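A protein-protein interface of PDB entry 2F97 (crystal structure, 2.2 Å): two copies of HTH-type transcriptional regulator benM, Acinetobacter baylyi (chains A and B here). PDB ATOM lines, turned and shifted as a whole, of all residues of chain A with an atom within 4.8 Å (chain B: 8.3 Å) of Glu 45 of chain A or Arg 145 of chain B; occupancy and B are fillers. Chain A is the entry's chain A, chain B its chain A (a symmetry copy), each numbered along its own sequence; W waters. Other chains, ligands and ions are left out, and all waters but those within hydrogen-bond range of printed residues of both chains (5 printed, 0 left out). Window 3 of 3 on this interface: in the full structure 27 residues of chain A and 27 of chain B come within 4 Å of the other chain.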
ATOM      1  N   PHE A  16      -3.348  22.652 -39.273  1.00  0.00           N
ATOM      2  CA  PHE A  16      -2.896  21.431 -38.604  1.00  0.00           C
ATOM      3  C   PHE A  16      -3.822  21.059 -37.447  1.00  0.00           C
ATOM      4  O   PHE A  16      -4.459  21.931 -36.846  1.00  0.00           O
ATOM      5  CB  PHE A  16      -1.460  21.610 -38.081  1.00  0.00           C
ATOM      6  CG  PHE A  16      -1.342  22.654 -37.002  1.00  0.00           C
ATOM      7  CD1 PHE A  16      -1.484  22.306 -35.659  1.00  0.00           C
ATOM      8  CD2 PHE A  16      -1.121  23.990 -37.328  1.00  0.00           C
ATOM      9  CE1 PHE A  16      -1.398  23.269 -34.659  1.00  0.00           C
ATOM     10  CE2 PHE A  16      -1.032  24.962 -36.333  1.00  0.00           C
ATOM     11  CZ  PHE A  16      -1.170  24.601 -34.999  1.00  0.00           C
ATOM     12  N   GLY A  18      -4.052  19.492 -33.552  1.00  0.00           N
ATOM     13  CA  GLY A  18      -3.210  19.587 -32.357  1.00  0.00           C
ATOM     14  C   GLY A  18      -2.426  18.339 -31.995  1.00  0.00           C
ATOM     15  O   GLY A  18      -1.345  18.434 -31.415  1.00  0.00           O
ATOM     16  N   LEU A  43       0.350  29.785 -38.989  1.00  0.00           N
ATOM     17  CA  LEU A  43      -0.057  28.458 -38.546  1.00  0.00           C
ATOM     18  C   LEU A  43      -1.422  28.518 -37.871  1.00  0.00           C
ATOM     19  O   LEU A  43      -1.640  29.334 -36.974  1.00  0.00           O
ATOM     20  CB  LEU A  43       0.998  27.868 -37.603  1.00  0.00           C
ATOM     21  CG  LEU A  43       2.422  27.785 -38.175  1.00  0.00           C
ATOM     22  CD1 LEU A  43       3.442  27.486 -37.085  1.00  0.00           C
ATOM     23  CD2 LEU A  43       2.519  26.756 -39.303  1.00  0.00           C
ATOM     24  N   TYR A  44      -2.336  27.659 -38.318  1.00  0.00           N
ATOM     25  CA  TYR A  44      -3.706  27.652 -37.815  1.00  0.00           C
ATOM     26  C   TYR A  44      -4.129  26.261 -37.368  1.00  0.00           C
ATOM     27  O   TYR A  44      -4.068  25.312 -38.149  1.00  0.00           O
ATOM     28  CB  TYR A  44      -4.679  28.148 -38.888  1.00  0.00           C
ATOM     29  CG  TYR A  44      -4.448  29.572 -39.325  1.00  0.00           C
ATOM     30  CD1 TYR A  44      -4.946  30.641 -38.579  1.00  0.00           C
ATOM     31  CD2 TYR A  44      -3.732  29.854 -40.489  1.00  0.00           C
ATOM     32  CE1 TYR A  44      -4.734  31.954 -38.981  1.00  0.00           C
ATOM     33  CE2 TYR A  44      -3.517  31.160 -40.899  1.00  0.00           C
ATOM     34  CZ  TYR A  44      -4.019  32.204 -40.141  1.00  0.00           C
ATOM     35  OH  TYR A  44      -3.808  33.499 -40.543  1.00  0.00           O
ATOM     36  N   GLU A  45      -4.559  26.149 -36.114  1.00  0.00           N
ATOM     37  CA  GLU A  45      -5.115  24.902 -35.606  1.00  0.00           C
ATOM     38  C   GLU A  45      -6.539  24.744 -36.133  1.00  0.00           C
ATOM     39  O   GLU A  45      -7.387  25.615 -35.924  1.00  0.00           O
ATOM     40  CB  GLU A  45      -5.109  24.881 -34.074  1.00  0.00           C
ATOM     41  CG  GLU A  45      -5.514  23.532 -33.469  1.00  0.00           C
ATOM     42  CD  GLU A  45      -5.959  23.620 -32.015  1.00  0.00           C
ATOM     43  OE1 GLU A  45      -6.272  24.729 -31.530  1.00  0.00           O
ATOM     44  OE2 GLU A  45      -6.014  22.563 -31.353  1.00  0.00           O
ATOM     45  N   MET A  46      -6.787  23.638 -36.827  1.00  0.00           N
ATOM     46  CA  MET A  46      -8.117  23.340 -37.368  1.00  0.00           C
ATOM     47  C   MET A  46      -8.257  21.870 -37.725  1.00  0.00           C
ATOM     48  O   MET A  46      -7.289  21.224 -38.131  1.00  0.00           O
ATOM     49  CB  MET A  46      -8.453  24.226 -38.588  1.00  0.00           C
ATOM     50  CG  MET A  46      -7.355  24.347 -39.630  1.00  0.00           C
ATOM     51  SD  MET A  46      -7.837  25.214 -41.150  1.00  0.00           S
ATOM     52  CE  MET A  46      -7.869  26.921 -40.621  1.00  0.00           C
ATOM     53  N   GLY A  47      -9.471  21.350 -37.564  1.00  0.00           N
ATOM     54  CA  GLY A  47      -9.792  19.982 -37.955  1.00  0.00           C
ATOM     55  C   GLY A  47      -9.775  19.836 -39.464  1.00  0.00           C
ATOM     56  O   GLY A  47      -9.765  20.836 -40.190  1.00  0.00           O
ATOM     57  N   ARG A 145     -12.350  16.890 -23.106  1.00  0.00           N
ATOM     58  CA  ARG A 145     -12.098  18.080 -23.919  1.00  0.00           C
ATOM     59  C   ARG A 145     -10.809  18.041 -24.743  1.00  0.00           C
ATOM     60  O   ARG A 145     -10.822  18.412 -25.914  1.00  0.00           O
ATOM     61  CB  ARG A 145     -12.142  19.342 -23.050  1.00  0.00           C
ATOM     62  CG  ARG A 145     -12.265  20.639 -23.843  1.00  0.00           C
ATOM     63  CD  ARG A 145     -12.268  21.852 -22.926  1.00  0.00           C
ATOM     64  NE  ARG A 145     -11.006  21.980 -22.201  1.00  0.00           N
ATOM     65  CZ  ARG A 145      -9.947  22.653 -22.641  1.00  0.00           C
ATOM     66  NH1 ARG A 145      -9.981  23.271 -23.817  1.00  0.00           N
ATOM     67  NH2 ARG A 145      -8.846  22.701 -21.904  1.00  0.00           N
ATOM     68  N   GLU A 146      -9.711  17.601 -24.126  1.00  0.00           N
ATOM     69  CA  GLU A 146      -8.376  17.659 -24.734  1.00  0.00           C
ATOM     70  C   GLU A 146      -7.515  16.463 -24.313  1.00  0.00           C
ATOM     71  O   GLU A 146      -7.816  15.788 -23.323  1.00  0.00           O
ATOM     72  CB  GLU A 146      -7.659  18.958 -24.332  1.00  0.00           C
ATOM     73  CG  GLU A 146      -8.269  20.262 -24.874  1.00  0.00           C
ATOM     74  CD  GLU A 146      -8.214  20.375 -26.393  1.00  0.00           C
ATOM     75  OE1 GLU A 146      -7.196  19.958 -26.992  1.00  0.00           O
ATOM     76  OE2 GLU A 146      -9.194  20.887 -26.986  1.00  0.00           O
ATOM     77  N   LEU B 113       4.046  33.764 -26.250  1.00  0.00           N
ATOM     78  CA  LEU B 113       2.805  33.024 -26.436  1.00  0.00           C
ATOM     79  C   LEU B 113       2.114  32.775 -25.102  1.00  0.00           C
ATOM     80  O   LEU B 113       2.637  32.066 -24.234  1.00  0.00           O
ATOM     81  CB  LEU B 113       3.051  31.709 -27.194  1.00  0.00           C
ATOM     82  CG  LEU B 113       3.704  31.855 -28.578  1.00  0.00           C
ATOM     83  CD1 LEU B 113       4.195  30.516 -29.101  1.00  0.00           C
ATOM     84  CD2 LEU B 113       2.766  32.515 -29.584  1.00  0.00           C
ATOM     85  N   LEU B 114       0.942  33.385 -24.948  1.00  0.00           N
ATOM     86  CA  LEU B 114       0.108  33.208 -23.767  1.00  0.00           C
ATOM     87  C   LEU B 114      -0.951  32.152 -24.047  1.00  0.00           C
ATOM     88  O   LEU B 114      -1.309  31.915 -25.200  1.00  0.00           O
ATOM     89  CB  LEU B 114      -0.563  34.530 -23.362  1.00  0.00           C
ATOM     90  CG  LEU B 114       0.289  35.783 -23.116  1.00  0.00           C
ATOM     91  CD1 LEU B 114      -0.609  36.999 -22.900  1.00  0.00           C
ATOM     92  CD2 LEU B 114       1.251  35.613 -21.943  1.00  0.00           C
ATOM     93  N   TYR B 115      -1.442  31.526 -22.981  1.00  0.00           N
ATOM     94  CA  TYR B 115      -2.444  30.469 -23.054  1.00  0.00           C
ATOM     95  C   TYR B 115      -3.063  30.326 -21.660  1.00  0.00           C
ATOM     96  O   TYR B 115      -2.458  30.755 -20.680  1.00  0.00           O
ATOM     97  CB  TYR B 115      -1.790  29.141 -23.473  1.00  0.00           C
ATOM     98  CG  TYR B 115      -0.866  28.563 -22.423  1.00  0.00           C
ATOM     99  CD1 TYR B 115      -1.356  27.718 -21.420  1.00  0.00           C
ATOM    100  CD2 TYR B 115       0.495  28.872 -22.421  1.00  0.00           C
ATOM    101  CE1 TYR B 115      -0.516  27.196 -20.447  1.00  0.00           C
ATOM    102  CE2 TYR B 115       1.348  28.351 -21.451  1.00  0.00           C
ATOM    103  CZ  TYR B 115       0.834  27.514 -20.469  1.00  0.00           C
ATOM    104  OH  TYR B 115       1.666  26.996 -19.509  1.00  0.00           O
ATOM    105  N   PRO B 116      -4.271  29.736 -21.560  1.00  0.00           N
ATOM    106  CA  PRO B 116      -5.165  29.323 -22.637  1.00  0.00           C
ATOM    107  C   PRO B 116      -6.089  30.471 -23.056  1.00  0.00           C
ATOM    108  O   PRO B 116      -5.936  31.588 -22.563  1.00  0.00           O
ATOM    109  CB  PRO B 116      -5.974  28.195 -21.992  1.00  0.00           C
ATOM    110  CG  PRO B 116      -6.069  28.588 -20.552  1.00  0.00           C
ATOM    111  CD  PRO B 116      -4.830  29.402 -20.232  1.00  0.00           C
ATOM    112  N   SER B 117      -7.035  30.192 -23.947  1.00  0.00           N
ATOM    113  CA  SER B 117      -7.988  31.206 -24.396  1.00  0.00           C
ATOM    114  C   SER B 117      -9.378  31.004 -23.783  1.00  0.00           C
ATOM    115  O   SER B 117     -10.382  31.480 -24.321  1.00  0.00           O
ATOM    116  CB  SER B 117      -8.067  31.225 -25.925  1.00  0.00           C
ATOM    117  OG  SER B 117      -8.556  29.992 -26.414  1.00  0.00           O
ATOM    118  N   SER B 118      -9.421  30.309 -22.651  1.00  0.00           N
ATOM    119  CA  SER B 118     -10.666  30.011 -21.945  1.00  0.00           C
ATOM    120  C   SER B 118     -11.126  31.202 -21.083  1.00  0.00           C
ATOM    121  O   SER B 118     -10.421  32.214 -21.016  1.00  0.00           O
ATOM    122  CB  SER B 118     -10.469  28.762 -21.083  1.00  0.00           C
ATOM    123  OG  SER B 118      -9.395  28.939 -20.186  1.00  0.00           O
ATOM    124  N   LYS B 120     -11.726  34.057 -18.475  1.00  0.00           N
ATOM    125  CA  LYS B 120     -10.782  34.742 -17.603  1.00  0.00           C
ATOM    126  C   LYS B 120     -11.354  34.836 -16.188  1.00  0.00           C
ATOM    127  O   LYS B 120     -12.573  34.825 -16.021  1.00  0.00           O
ATOM    128  CB  LYS B 120     -10.462  36.137 -18.159  1.00  0.00           C
ATOM    129  CG  LYS B 120      -9.832  36.144 -19.558  1.00  0.00           C
ATOM    130  CD  LYS B 120      -8.447  35.499 -19.566  1.00  0.00           C
ATOM    131  CE  LYS B 120      -7.758  35.639 -20.924  1.00  0.00           C
ATOM    132  NZ  LYS B 120      -8.284  34.686 -21.948  1.00  0.00           N
ATOM    133  N   ASN B 122      -7.400  33.320 -16.197  1.00  0.00           N
ATOM    134  CA  ASN B 122      -6.733  32.044 -16.421  1.00  0.00           C
ATOM    135  C   ASN B 122      -5.216  32.235 -16.350  1.00  0.00           C
ATOM    136  O   ASN B 122      -4.742  33.302 -15.943  1.00  0.00           O
ATOM    137  CB  ASN B 122      -7.174  31.416 -17.752  1.00  0.00           C
ATOM    138  CG  ASN B 122      -6.904  32.316 -18.951  1.00  0.00           C
ATOM    139  OD1 ASN B 122      -5.973  33.117 -18.951  1.00  0.00           O
ATOM    140  ND2 ASN B 122      -7.723  32.176 -19.986  1.00  0.00           N
ATOM    141  N   ASN B 142       0.824  37.063 -28.039  1.00  0.00           N
ATOM    142  CA  ASN B 142      -0.199  36.342 -28.781  1.00  0.00           C
ATOM    143  C   ASN B 142      -0.805  35.272 -27.881  1.00  0.00           C
ATOM    144  O   ASN B 142      -0.092  34.415 -27.357  1.00  0.00           O
ATOM    145  CB  ASN B 142       0.403  35.714 -30.045  1.00  0.00           C
ATOM    146  CG  ASN B 142      -0.615  34.927 -30.866  1.00  0.00           C
ATOM    147  OD1 ASN B 142      -0.293  33.873 -31.415  1.00  0.00           O
ATOM    148  ND2 ASN B 142      -1.838  35.440 -30.962  1.00  0.00           N
ATOM    149  N   GLU B 143      -2.118  35.340 -27.691  1.00  0.00           N
ATOM    150  CA  GLU B 143      -2.820  34.346 -26.894  1.00  0.00           C
ATOM    151  C   GLU B 143      -3.229  33.185 -27.788  1.00  0.00           C
ATOM    152  O   GLU B 143      -3.931  33.371 -28.782  1.00  0.00           O
ATOM    153  CB  GLU B 143      -4.035  34.961 -26.192  1.00  0.00           C
ATOM    154  CG  GLU B 143      -4.715  34.019 -25.199  1.00  0.00           C
ATOM    155  CD  GLU B 143      -5.623  34.752 -24.229  1.00  0.00           C
ATOM    156  OE1 GLU B 143      -5.102  35.354 -23.262  1.00  0.00           O
ATOM    157  OE2 GLU B 143      -6.855  34.721 -24.429  1.00  0.00           O
ATOM    158  N   VAL B 144      -2.759  31.991 -27.438  1.00  0.00           N
ATOM    159  CA  VAL B 144      -3.132  30.777 -28.155  1.00  0.00           C
ATOM    160  C   VAL B 144      -4.071  29.922 -27.298  1.00  0.00           C
ATOM    161  O   VAL B 144      -4.226  30.168 -26.094  1.00  0.00           O
ATOM    162  CB  VAL B 144      -1.897  29.984 -28.673  1.00  0.00           C
ATOM    163  CG1 VAL B 144      -1.105  30.829 -29.670  1.00  0.00           C
ATOM    164  CG2 VAL B 144      -1.011  29.514 -27.525  1.00  0.00           C
ATOM    165  N   ARG B 145      -4.686  28.923 -27.924  1.00  0.00           N
ATOM    166  CA  ARG B 145      -5.810  28.203 -27.326  1.00  0.00           C
ATOM    167  C   ARG B 145      -5.459  27.359 -26.098  1.00  0.00           C
ATOM    168  O   ARG B 145      -6.188  27.387 -25.109  1.00  0.00           O
ATOM    169  CB  ARG B 145      -6.520  27.347 -28.380  1.00  0.00           C
ATOM    170  CG  ARG B 145      -7.903  26.860 -27.957  1.00  0.00           C
ATOM    171  CD  ARG B 145      -8.538  25.991 -29.031  1.00  0.00           C
ATOM    172  NE  ARG B 145      -7.769  24.769 -29.257  1.00  0.00           N
ATOM    173  CZ  ARG B 145      -7.956  23.627 -28.603  1.00  0.00           C
ATOM    174  NH1 ARG B 145      -8.894  23.532 -27.666  1.00  0.00           N
ATOM    175  NH2 ARG B 145      -7.197  22.577 -28.881  1.00  0.00           N
ATOM    176  N   GLU B 146      -4.355  26.613 -26.174  1.00  0.00           N
ATOM    177  CA  GLU B 146      -3.980  25.634 -25.145  1.00  0.00           C
ATOM    178  C   GLU B 146      -2.459  25.547 -24.980  1.00  0.00           C
ATOM    179  O   GLU B 146      -1.705  25.979 -25.859  1.00  0.00           O
ATOM    180  CB  GLU B 146      -4.525  24.242 -25.504  1.00  0.00           C
ATOM    181  CG  GLU B 146      -6.056  24.091 -25.489  1.00  0.00           C
ATOM    182  CD  GLU B 146      -6.673  24.281 -24.109  1.00  0.00           C
ATOM    183  OE1 GLU B 146      -6.069  23.824 -23.110  1.00  0.00           O
ATOM    184  OE2 GLU B 146      -7.768  24.886 -24.025  1.00  0.00           O
ATOM    185  N   VAL B 147      -2.021  24.962 -23.867  1.00  0.00           N
ATOM    186  CA  VAL B 147      -0.593  24.800 -23.564  1.00  0.00           C
ATOM    187  C   VAL B 147       0.201  24.108 -24.685  1.00  0.00           C
ATOM    188  O   VAL B 147       1.286  24.570 -25.042  1.00  0.00           O
ATOM    189  CB  VAL B 147      -0.353  24.099 -22.190  1.00  0.00           C
ATOM    190  CG1 VAL B 147      -0.894  22.666 -22.179  1.00  0.00           C
ATOM    191  CG2 VAL B 147       1.130  24.130 -21.818  1.00  0.00           C
ATOM    192  N   GLN B 148      -0.348  23.025 -25.243  1.00  0.00           N
ATOM    193  CA  GLN B 148       0.343  22.266 -26.294  1.00  0.00           C
ATOM    194  C   GLN B 148       0.507  23.068 -27.581  1.00  0.00           C
ATOM    195  O   GLN B 148       1.455  22.839 -28.337  1.00  0.00           O
ATOM    196  CB  GLN B 148      -0.339  20.919 -26.582  1.00  0.00           C
ATOM    197  CG  GLN B 148      -1.752  20.998 -27.164  1.00  0.00           C
ATOM    198  CD  GLN B 148      -2.843  20.964 -26.100  1.00  0.00           C
ATOM    199  OE1 GLN B 148      -2.669  21.463 -24.986  1.00  0.00           O
ATOM    200  NE2 GLN B 148      -3.981  20.375 -26.449  1.00  0.00           N
ATOM    201  N   LEU B 149      -0.416  23.998 -27.825  1.00  0.00           N
ATOM    202  CA  LEU B 149      -0.320  24.892 -28.970  1.00  0.00           C
ATOM    203  C   LEU B 149       0.819  25.888 -28.757  1.00  0.00           C
ATOM    204  O   LEU B 149       1.599  26.137 -29.671  1.00  0.00           O
ATOM    205  CB  LEU B 149      -1.646  25.619 -29.225  1.00  0.00           C
ATOM    206  CG  LEU B 149      -1.925  26.023 -30.677  1.00  0.00           C
ATOM    207  CD1 LEU B 149      -2.382  24.829 -31.497  1.00  0.00           C
ATOM    208  CD2 LEU B 149      -2.971  27.108 -30.739  1.00  0.00           C
ATOM    209  N   ALA B 150       0.916  26.430 -27.544  1.00  0.00           N
ATOM    210  CA  ALA B 150       2.015  27.325 -27.164  1.00  0.00           C
ATOM    211  C   ALA B 150       3.373  26.637 -27.309  1.00  0.00           C
ATOM    212  O   ALA B 150       4.268  27.162 -27.969  1.00  0.00           O
ATOM    213  CB  ALA B 150       1.825  27.838 -25.736  1.00  0.00           C
ATOM    214  N   LEU B 153       4.181  25.602 -31.039  1.00  0.00           N
ATOM    215  CA  LEU B 153       4.554  26.769 -31.839  1.00  0.00           C
ATOM    216  C   LEU B 153       5.954  27.282 -31.502  1.00  0.00           C
ATOM    217  O   LEU B 153       6.684  27.716 -32.394  1.00  0.00           O
ATOM    218  CB  LEU B 153       3.515  27.890 -31.701  1.00  0.00           C
ATOM    219  CG  LEU B 153       2.122  27.641 -32.303  1.00  0.00           C
ATOM    220  CD1 LEU B 153       1.125  28.690 -31.823  1.00  0.00           C
ATOM    221  CD2 LEU B 153       2.160  27.589 -33.822  1.00  0.00           C
HETATM  222  O   HOH W   1      -4.934  20.357 -29.364  1.00  0.00           O
HETATM  223  O   HOH W   2      -9.439  20.337 -30.126  1.00  0.00           O
HETATM  224  O   HOH W   3      -3.266  18.404 -28.839  1.00  0.00           O
HETATM  225  O   HOH W   4      -6.164  22.258 -20.205  1.00  0.00           O
HETATM  226  O   HOH W   5      -8.592  26.011 -21.148  1.00  0.00           O
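The side-chain carboxylate (OE1) of Glu 45 of chain A lies within salt-bridge range of the guanidinium group (NE) of Arg 145 of chain B (2.7 Å).
The guanidinium group (NH1) of Arg 145 of chain A is in salt-bridge range of the side-chain carboxylate (OE2) of Glu 146 of chain B.
The guanidinium group of Arg 145 of chain B is in salt-bridge range of the side-chain carboxylate of Glu 146 of chain A, at 2.7 Å.
The side-chain carboxylate of Glu 146 of chain A is in hydrogen-bond range of the side-chain amide nitrogen of Gln 148 of chain B (3.3 Å).
O of Tyr 44 of chain A is in hydrogen-bond range of N of Phe 16 of chain A (3.0 Å).
O of Phe 16 of chain A sits at hydrogen-bond distance from N of Met 46 of chain A (2.9 Å).
N of Ser 117 of chain B is in hydrogen-bond range of O of Arg 145 of chain B, at 3.2 Å.
CD1 of Leu 149 of chain B touches CE1 of Phe 16 of chain A, at 3.7 Å.
Leu 153 of chain B touches Leu 43 of chain A (CD2 to CD1, 3.5 Å).
Leu 149 of chain B touches Glu 45 of chain A (CD1 to CB, 3.8 Å).
Of the printed residues of chain B, Glu 45 of chain A touches Arg 145 and Leu 149.
Printed residues of chain A within 4 Å of Arg 145 of chain B: Glu 45 and Glu 146.
Of the printed residues of chain A, Leu 149 of chain B touches Phe 16 and Glu 45.
Of the printed residues of chain B, Arg 145 of chain A touches Glu 146 (2.7 Å).
Of the printed residues of chain B, Leu 43 of chain A touches Leu 153 (3.5 Å).
Pro 116 of chain B touches none of the printed residues of chain A.
The nearest printed residue of chain A that does not touch Leu 153 of chain B is Phe 16 of chain A (4.6 Å).
Hydrophobic or aromatic side chains of chain A that line the printed part of chain B: Phe 16 and Leu 43.
Printed residues of chain B that touch a printed residue of chain A: Arg 145, Glu 146, Gln 148, Leu 149 and Leu 153.
Among the printed residues, Asp or Glu carboxylates within 4 Å of a Lys or Arg side-chain nitrogen of the other chain: Glu 45 of chain A with Arg 145 of chain B (2.7 Å), Arg 145 of chain A with Glu 146 of chain B (2.7 Å) and Glu 146 of chain A with Arg 145 of chain B (2.7 Å).
Arg 145 of chain A touches Glu 146 of chain B, and with the chains exchanged Glu 146 of chain A touches Arg 145 of chain B.
Positions printed for both chains: 145 and 146.
Of the 7 pairs that touch across the chains among the printed residues, 2 have their exchanged pair printed and touching as well.
Water W1 lies within hydrogen-bond range of NE2 of Gln 148 of chain B (3.1 Å), OE2 of Glu 45 of chain A (3.2 Å), NH2 of Arg 145 of chain B (3.2 Å) and OE1 of Glu 146 of chain A (3.3 Å).
Water W3 bridges the side-chain amide nitrogen of Gln 148 of chain B (3.2 Å) and the backbone carbonyl oxygen of Gly 18 of chain A (3.2 Å).
Water W5 lies within hydrogen-bond range of OG of Ser 118 of chain B (3.2 Å), OE2 of Glu 146 of chain B (3.2 Å) and NH2 of Arg 145 of chain A (3.4 Å).
Water W2 lies within hydrogen-bond range of the side-chain carboxylate of Glu 146 of chain A and the guanidinium group of Arg 145 of chain B.
Water W4 lies within hydrogen-bond range of NH2 of Arg 145 of chain A (3.2 Å) and OE1 of Glu 146 of chain B (3.3 Å).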
